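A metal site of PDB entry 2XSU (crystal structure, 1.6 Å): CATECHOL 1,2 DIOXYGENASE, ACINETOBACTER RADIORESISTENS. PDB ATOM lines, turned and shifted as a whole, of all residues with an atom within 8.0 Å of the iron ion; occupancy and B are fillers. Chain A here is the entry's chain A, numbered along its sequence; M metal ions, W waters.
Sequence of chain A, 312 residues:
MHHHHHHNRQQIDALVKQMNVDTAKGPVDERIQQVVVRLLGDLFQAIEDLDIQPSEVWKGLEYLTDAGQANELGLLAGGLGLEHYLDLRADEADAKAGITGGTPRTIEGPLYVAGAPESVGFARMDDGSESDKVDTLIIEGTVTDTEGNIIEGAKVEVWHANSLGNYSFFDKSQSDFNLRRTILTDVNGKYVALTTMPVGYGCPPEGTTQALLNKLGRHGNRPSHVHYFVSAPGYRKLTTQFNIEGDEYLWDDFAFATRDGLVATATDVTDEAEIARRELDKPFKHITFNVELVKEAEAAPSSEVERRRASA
N of His 227 is in hydrogen-bond range of O of Trp 159 (3.0 Å).
ND1 of His 227 lies close to O of Glu 108 (3.2 Å).
A ring nitrogen (ND1) of His 225 lies within hydrogen-bond range of the backbone carbonyl oxygen (O) of Pro 223 (2.8 Å).
The backbone carbonyl oxygen (O) of Tyr 201 sits at hydrogen-bond distance from the backbone NH (N) of Arg 222 (2.9 Å).
Residues that only touch the iron ion: Arg 222.
Of the 20 residues printed, 5 come within 4 Å of the iron ion.
The iron ion is bound by OH of Tyr 167 (1.9 Å), NE2 of His 227 (2.1 Å), NE2 of His 225 (2.1 Å), water W1 (2.1 Å) and OH of Tyr 201 (2.4 Å).
The iron ion has five donor atoms within binding distance.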
ATOM      1  N   ILE A 107      17.887  25.164  32.754  1.00  0.00           N
ATOM      2  CA  ILE A 107      17.369  26.535  32.885  1.00  0.00           C
ATOM      3  C   ILE A 107      15.852  26.612  32.793  1.00  0.00           C
ATOM      4  O   ILE A 107      15.206  25.804  32.076  1.00  0.00           O
ATOM      5  CB  ILE A 107      18.018  27.494  31.886  1.00  0.00           C
ATOM      6  CG1 ILE A 107      17.524  27.227  30.469  1.00  0.00           C
ATOM      7  CG2 ILE A 107      19.549  27.398  32.018  1.00  0.00           C
ATOM      8  CD1 ILE A 107      18.047  28.305  29.427  1.00  0.00           C
ATOM      9  N   GLU A 108      15.285  27.554  33.537  1.00  0.00           N
ATOM     10  CA  GLU A 108      13.839  27.815  33.482  1.00  0.00           C
ATOM     11  C   GLU A 108      13.430  28.506  32.172  1.00  0.00           C
ATOM     12  O   GLU A 108      12.338  28.240  31.670  1.00  0.00           O
ATOM     13  CB  GLU A 108      13.466  28.721  34.659  1.00  0.00           C
ATOM     14  CG  GLU A 108      11.969  28.974  34.848  1.00  0.00           C
ATOM     15  CD  GLU A 108      11.688  29.866  36.064  1.00  0.00           C
ATOM     16  OE1 GLU A 108      12.384  29.730  37.101  1.00  0.00           O
ATOM     17  OE2 GLU A 108      10.739  30.698  36.000  1.00  0.00           O
ATOM     18  N   GLY A 109      14.276  29.401  31.644  1.00  0.00           N
ATOM     19  CA  GLY A 109      13.852  30.307  30.585  1.00  0.00           C
ATOM     20  C   GLY A 109      12.961  31.402  31.152  1.00  0.00           C
ATOM     21  O   GLY A 109      12.599  31.369  32.341  1.00  0.00           O
ATOM     22  N   PRO A 110      12.580  32.359  30.305  1.00  0.00           N
ATOM     23  CA  PRO A 110      11.837  33.516  30.769  1.00  0.00           C
ATOM     24  C   PRO A 110      10.344  33.461  30.566  1.00  0.00           C
ATOM     25  O   PRO A 110       9.676  34.506  30.748  1.00  0.00           O
ATOM     26  CB  PRO A 110      12.440  34.641  29.918  1.00  0.00           C
ATOM     27  CG  PRO A 110      12.716  34.012  28.604  1.00  0.00           C
ATOM     28  CD  PRO A 110      13.137  32.558  28.957  1.00  0.00           C
ATOM     29  N   LEU A 111       9.790  32.288  30.219  1.00  0.00           N
ATOM     30  CA  LEU A 111       8.407  32.253  29.700  1.00  0.00           C
ATOM     31  C   LEU A 111       7.399  31.442  30.557  1.00  0.00           C
ATOM     32  O   LEU A 111       6.289  31.113  30.088  1.00  0.00           O
ATOM     33  CB  LEU A 111       8.376  31.784  28.233  1.00  0.00           C
ATOM     34  CG  LEU A 111       9.280  32.583  27.287  1.00  0.00           C
ATOM     35  CD1 LEU A 111       9.225  31.971  25.871  1.00  0.00           C
ATOM     36  CD2 LEU A 111       8.934  34.068  27.287  1.00  0.00           C
ATOM     37  N   TYR A 112       7.761  31.139  31.803  1.00  0.00           N
ATOM     38  CA  TYR A 112       6.766  30.568  32.721  1.00  0.00           C
ATOM     39  C   TYR A 112       5.626  31.542  33.019  1.00  0.00           C
ATOM     40  O   TYR A 112       5.864  32.742  33.158  1.00  0.00           O
ATOM     41  CB  TYR A 112       7.413  30.108  34.028  1.00  0.00           C
ATOM     42  CG  TYR A 112       6.432  29.560  35.051  1.00  0.00           C
ATOM     43  CD1 TYR A 112       5.919  28.262  34.937  1.00  0.00           C
ATOM     44  CD2 TYR A 112       6.034  30.341  36.135  1.00  0.00           C
ATOM     45  CE1 TYR A 112       5.020  27.760  35.885  1.00  0.00           C
ATOM     46  CE2 TYR A 112       5.157  29.856  37.096  1.00  0.00           C
ATOM     47  CZ  TYR A 112       4.647  28.567  36.980  1.00  0.00           C
ATOM     48  OH  TYR A 112       3.778  28.079  37.944  1.00  0.00           O
ATOM     49  N   TRP A 159       5.175  23.434  30.365  1.00  0.00           N
ATOM     50  CA  TRP A 159       4.849  24.432  29.352  1.00  0.00           C
ATOM     51  C   TRP A 159       5.772  24.280  28.156  1.00  0.00           C
ATOM     52  O   TRP A 159       6.937  23.902  28.304  1.00  0.00           O
ATOM     53  CB  TRP A 159       4.833  25.882  29.937  1.00  0.00           C
ATOM     54  CG  TRP A 159       6.195  26.484  30.427  1.00  0.00           C
ATOM     55  CD1 TRP A 159       6.933  27.450  29.790  1.00  0.00           C
ATOM     56  CD2 TRP A 159       6.892  26.186  31.654  1.00  0.00           C
ATOM     57  NE1 TRP A 159       8.060  27.756  30.546  1.00  0.00           N
ATOM     58  CE2 TRP A 159       8.061  27.001  31.689  1.00  0.00           C
ATOM     59  CE3 TRP A 159       6.663  25.292  32.718  1.00  0.00           C
ATOM     60  CZ2 TRP A 159       8.997  26.940  32.751  1.00  0.00           C
ATOM     61  CZ3 TRP A 159       7.578  25.226  33.775  1.00  0.00           C
ATOM     62  CH2 TRP A 159       8.752  26.067  33.784  1.00  0.00           C
ATOM     63  N   HIS A 160       5.244  24.573  26.976  1.00  0.00           N
ATOM     64  CA  HIS A 160       6.056  24.440  25.735  1.00  0.00           C
ATOM     65  C   HIS A 160       5.443  25.255  24.584  1.00  0.00           C
ATOM     66  O   HIS A 160       4.305  25.772  24.697  1.00  0.00           O
ATOM     67  CB  HIS A 160       6.264  22.962  25.368  1.00  0.00           C
ATOM     68  CG  HIS A 160       5.057  22.233  24.865  1.00  0.00           C
ATOM     69  ND1 HIS A 160       4.540  22.411  23.588  1.00  0.00           N
ATOM     70  CD2 HIS A 160       4.298  21.275  25.441  1.00  0.00           C
ATOM     71  CE1 HIS A 160       3.494  21.609  23.422  1.00  0.00           C
ATOM     72  NE2 HIS A 160       3.345  20.898  24.526  1.00  0.00           N
ATOM     73  N   ALA A 161       6.212  25.352  23.499  1.00  0.00           N
ATOM     74  CA  ALA A 161       5.851  26.095  22.284  1.00  0.00           C
ATOM     75  C   ALA A 161       4.878  25.350  21.358  1.00  0.00           C
ATOM     76  O   ALA A 161       4.823  24.087  21.336  1.00  0.00           O
ATOM     77  CB  ALA A 161       7.102  26.487  21.499  1.00  0.00           C
ATOM     78  N   GLY A 165       6.666  27.631  17.112  1.00  0.00           N
ATOM     79  CA  GLY A 165       7.679  28.001  18.099  1.00  0.00           C
ATOM     80  C   GLY A 165       7.275  29.133  19.032  1.00  0.00           C
ATOM     81  O   GLY A 165       8.146  29.754  19.642  1.00  0.00           O
ATOM     82  N   TYR A 167       4.813  30.755  22.360  1.00  0.00           N
ATOM     83  CA  TYR A 167       4.242  30.404  23.656  1.00  0.00           C
ATOM     84  C   TYR A 167       3.025  31.265  23.961  1.00  0.00           C
ATOM     85  O   TYR A 167       2.998  32.458  23.649  1.00  0.00           O
ATOM     86  CB  TYR A 167       5.269  30.680  24.754  1.00  0.00           C
ATOM     87  CG  TYR A 167       6.400  29.670  24.878  1.00  0.00           C
ATOM     88  CD1 TYR A 167       6.399  28.740  25.916  1.00  0.00           C
ATOM     89  CD2 TYR A 167       7.491  29.697  24.013  1.00  0.00           C
ATOM     90  CE1 TYR A 167       7.421  27.846  26.067  1.00  0.00           C
ATOM     91  CE2 TYR A 167       8.539  28.791  24.143  1.00  0.00           C
ATOM     92  CZ  TYR A 167       8.502  27.882  25.176  1.00  0.00           C
ATOM     93  OH  TYR A 167       9.540  26.996  25.351  1.00  0.00           O
ATOM     94  N   VAL A 199       8.107  22.790  18.391  1.00  0.00           N
ATOM     95  CA  VAL A 199       9.215  23.083  17.496  1.00  0.00           C
ATOM     96  C   VAL A 199      10.152  24.059  18.196  1.00  0.00           C
ATOM     97  O   VAL A 199       9.730  24.833  19.052  1.00  0.00           O
ATOM     98  CB  VAL A 199       8.669  23.632  16.152  1.00  0.00           C
ATOM     99  CG1 VAL A 199       8.203  25.040  16.287  1.00  0.00           C
ATOM    100  CG2 VAL A 199       9.704  23.515  15.073  1.00  0.00           C
ATOM    101  N   TYR A 201      12.792  27.279  18.243  1.00  0.00           N
ATOM    102  CA  TYR A 201      12.481  28.635  17.837  1.00  0.00           C
ATOM    103  C   TYR A 201      13.687  29.508  18.038  1.00  0.00           C
ATOM    104  O   TYR A 201      14.594  29.161  18.790  1.00  0.00           O
ATOM    105  CB  TYR A 201      11.310  29.145  18.697  1.00  0.00           C
ATOM    106  CG  TYR A 201      11.525  29.004  20.193  1.00  0.00           C
ATOM    107  CD1 TYR A 201      12.167  30.001  20.948  1.00  0.00           C
ATOM    108  CD2 TYR A 201      11.062  27.872  20.881  1.00  0.00           C
ATOM    109  CE1 TYR A 201      12.335  29.886  22.308  1.00  0.00           C
ATOM    110  CE2 TYR A 201      11.232  27.738  22.257  1.00  0.00           C
ATOM    111  CZ  TYR A 201      11.877  28.737  22.969  1.00  0.00           C
ATOM    112  OH  TYR A 201      12.067  28.626  24.334  1.00  0.00           O
ATOM    113  N   ARG A 222      16.917  27.795  19.850  1.00  0.00           N
ATOM    114  CA  ARG A 222      16.867  26.678  20.814  1.00  0.00           C
ATOM    115  C   ARG A 222      16.282  25.438  20.113  1.00  0.00           C
ATOM    116  O   ARG A 222      15.377  25.580  19.285  1.00  0.00           O
ATOM    117  CB  ARG A 222      15.989  27.008  22.020  1.00  0.00           C
ATOM    118  CG  ARG A 222      16.391  28.279  22.740  1.00  0.00           C
ATOM    119  CD  ARG A 222      15.951  28.245  24.163  1.00  0.00           C
ATOM    120  NE  ARG A 222      16.666  27.251  24.927  1.00  0.00           N
ATOM    121  CZ  ARG A 222      16.303  26.827  26.127  1.00  0.00           C
ATOM    122  NH1 ARG A 222      15.195  27.302  26.704  1.00  0.00           N
ATOM    123  NH2 ARG A 222      17.029  25.920  26.734  1.00  0.00           N
ATOM    124  N   PRO A 223      16.793  24.237  20.439  1.00  0.00           N
ATOM    125  CA  PRO A 223      16.130  22.996  19.972  1.00  0.00           C
ATOM    126  C   PRO A 223      14.780  22.852  20.638  1.00  0.00           C
ATOM    127  O   PRO A 223      14.521  23.460  21.717  1.00  0.00           O
ATOM    128  CB  PRO A 223      17.060  21.874  20.443  1.00  0.00           C
ATOM    129  CG  PRO A 223      17.640  22.447  21.754  1.00  0.00           C
ATOM    130  CD  PRO A 223      17.835  23.941  21.448  1.00  0.00           C
ATOM    131  N   SER A 224      13.925  22.025  20.040  1.00  0.00           N
ATOM    132  CA  SER A 224      12.605  21.699  20.631  1.00  0.00           C
ATOM    133  C   SER A 224      12.777  21.169  22.063  1.00  0.00           C
ATOM    134  O   SER A 224      13.744  20.424  22.376  1.00  0.00           O
ATOM    135  CB  SER A 224      11.907  20.646  19.801  1.00  0.00           C
ATOM    136  OG  SER A 224      12.735  19.498  19.772  1.00  0.00           O
ATOM    137  N   HIS A 225      11.851  21.571  22.952  1.00  0.00           N
ATOM    138  CA  HIS A 225      11.949  21.179  24.361  1.00  0.00           C
ATOM    139  C   HIS A 225      10.606  21.390  25.069  1.00  0.00           C
ATOM    140  O   HIS A 225       9.749  22.148  24.601  1.00  0.00           O
ATOM    141  CB  HIS A 225      13.029  22.020  25.111  1.00  0.00           C
ATOM    142  CG  HIS A 225      12.790  23.504  25.054  1.00  0.00           C
ATOM    143  ND1 HIS A 225      13.173  24.283  23.986  1.00  0.00           N
ATOM    144  CD2 HIS A 225      12.171  24.347  25.937  1.00  0.00           C
ATOM    145  CE1 HIS A 225      12.815  25.541  24.198  1.00  0.00           C
ATOM    146  NE2 HIS A 225      12.213  25.617  25.380  1.00  0.00           N
ATOM    147  N   VAL A 226      10.434  20.699  26.193  1.00  0.00           N
ATOM    148  CA  VAL A 226       9.285  20.918  27.078  1.00  0.00           C
ATOM    149  C   VAL A 226       9.833  21.239  28.475  1.00  0.00           C
ATOM    150  O   VAL A 226      10.705  20.527  28.999  1.00  0.00           O
ATOM    151  CB  VAL A 226       8.373  19.639  27.130  1.00  0.00           C
ATOM    152  CG1 VAL A 226       7.234  19.804  28.169  1.00  0.00           C
ATOM    153  CG2 VAL A 226       7.791  19.338  25.720  1.00  0.00           C
ATOM    154  N   HIS A 227       9.329  22.318  29.075  1.00  0.00           N
ATOM    155  CA  HIS A 227       9.775  22.766  30.391  1.00  0.00           C
ATOM    156  C   HIS A 227       9.020  22.041  31.507  1.00  0.00           C
ATOM    157  O   HIS A 227       7.821  21.769  31.351  1.00  0.00           O
ATOM    158  CB  HIS A 227       9.433  24.259  30.517  1.00  0.00           C
ATOM    159  CG  HIS A 227      10.224  25.158  29.634  1.00  0.00           C
ATOM    160  ND1 HIS A 227      11.474  25.614  29.982  1.00  0.00           N
ATOM    161  CD2 HIS A 227       9.946  25.738  28.428  1.00  0.00           C
ATOM    162  CE1 HIS A 227      11.943  26.417  29.036  1.00  0.00           C
ATOM    163  NE2 HIS A 227      11.057  26.486  28.060  1.00  0.00           N
ATOM    164  N   GLN A 241      13.961  20.252  31.942  1.00  0.00           N
ATOM    165  CA  GLN A 241      13.285  20.107  30.650  1.00  0.00           C
ATOM    166  C   GLN A 241      13.649  18.754  30.048  1.00  0.00           C
ATOM    167  O   GLN A 241      14.541  18.084  30.546  1.00  0.00           O
ATOM    168  CB  GLN A 241      13.699  21.189  29.674  1.00  0.00           C
ATOM    169  CG  GLN A 241      15.069  21.056  29.114  1.00  0.00           C
ATOM    170  CD  GLN A 241      15.449  22.225  28.214  1.00  0.00           C
ATOM    171  OE1 GLN A 241      14.745  23.256  28.166  1.00  0.00           O
ATOM    172  NE2 GLN A 241      16.566  22.066  27.508  1.00  0.00           N
HETATM  173 FE    FE M   1      11.267  27.340  26.172  1.00  0.00          FE
HETATM  174  O   HOH W   1      11.812  29.250  26.984  1.00  0.00           O
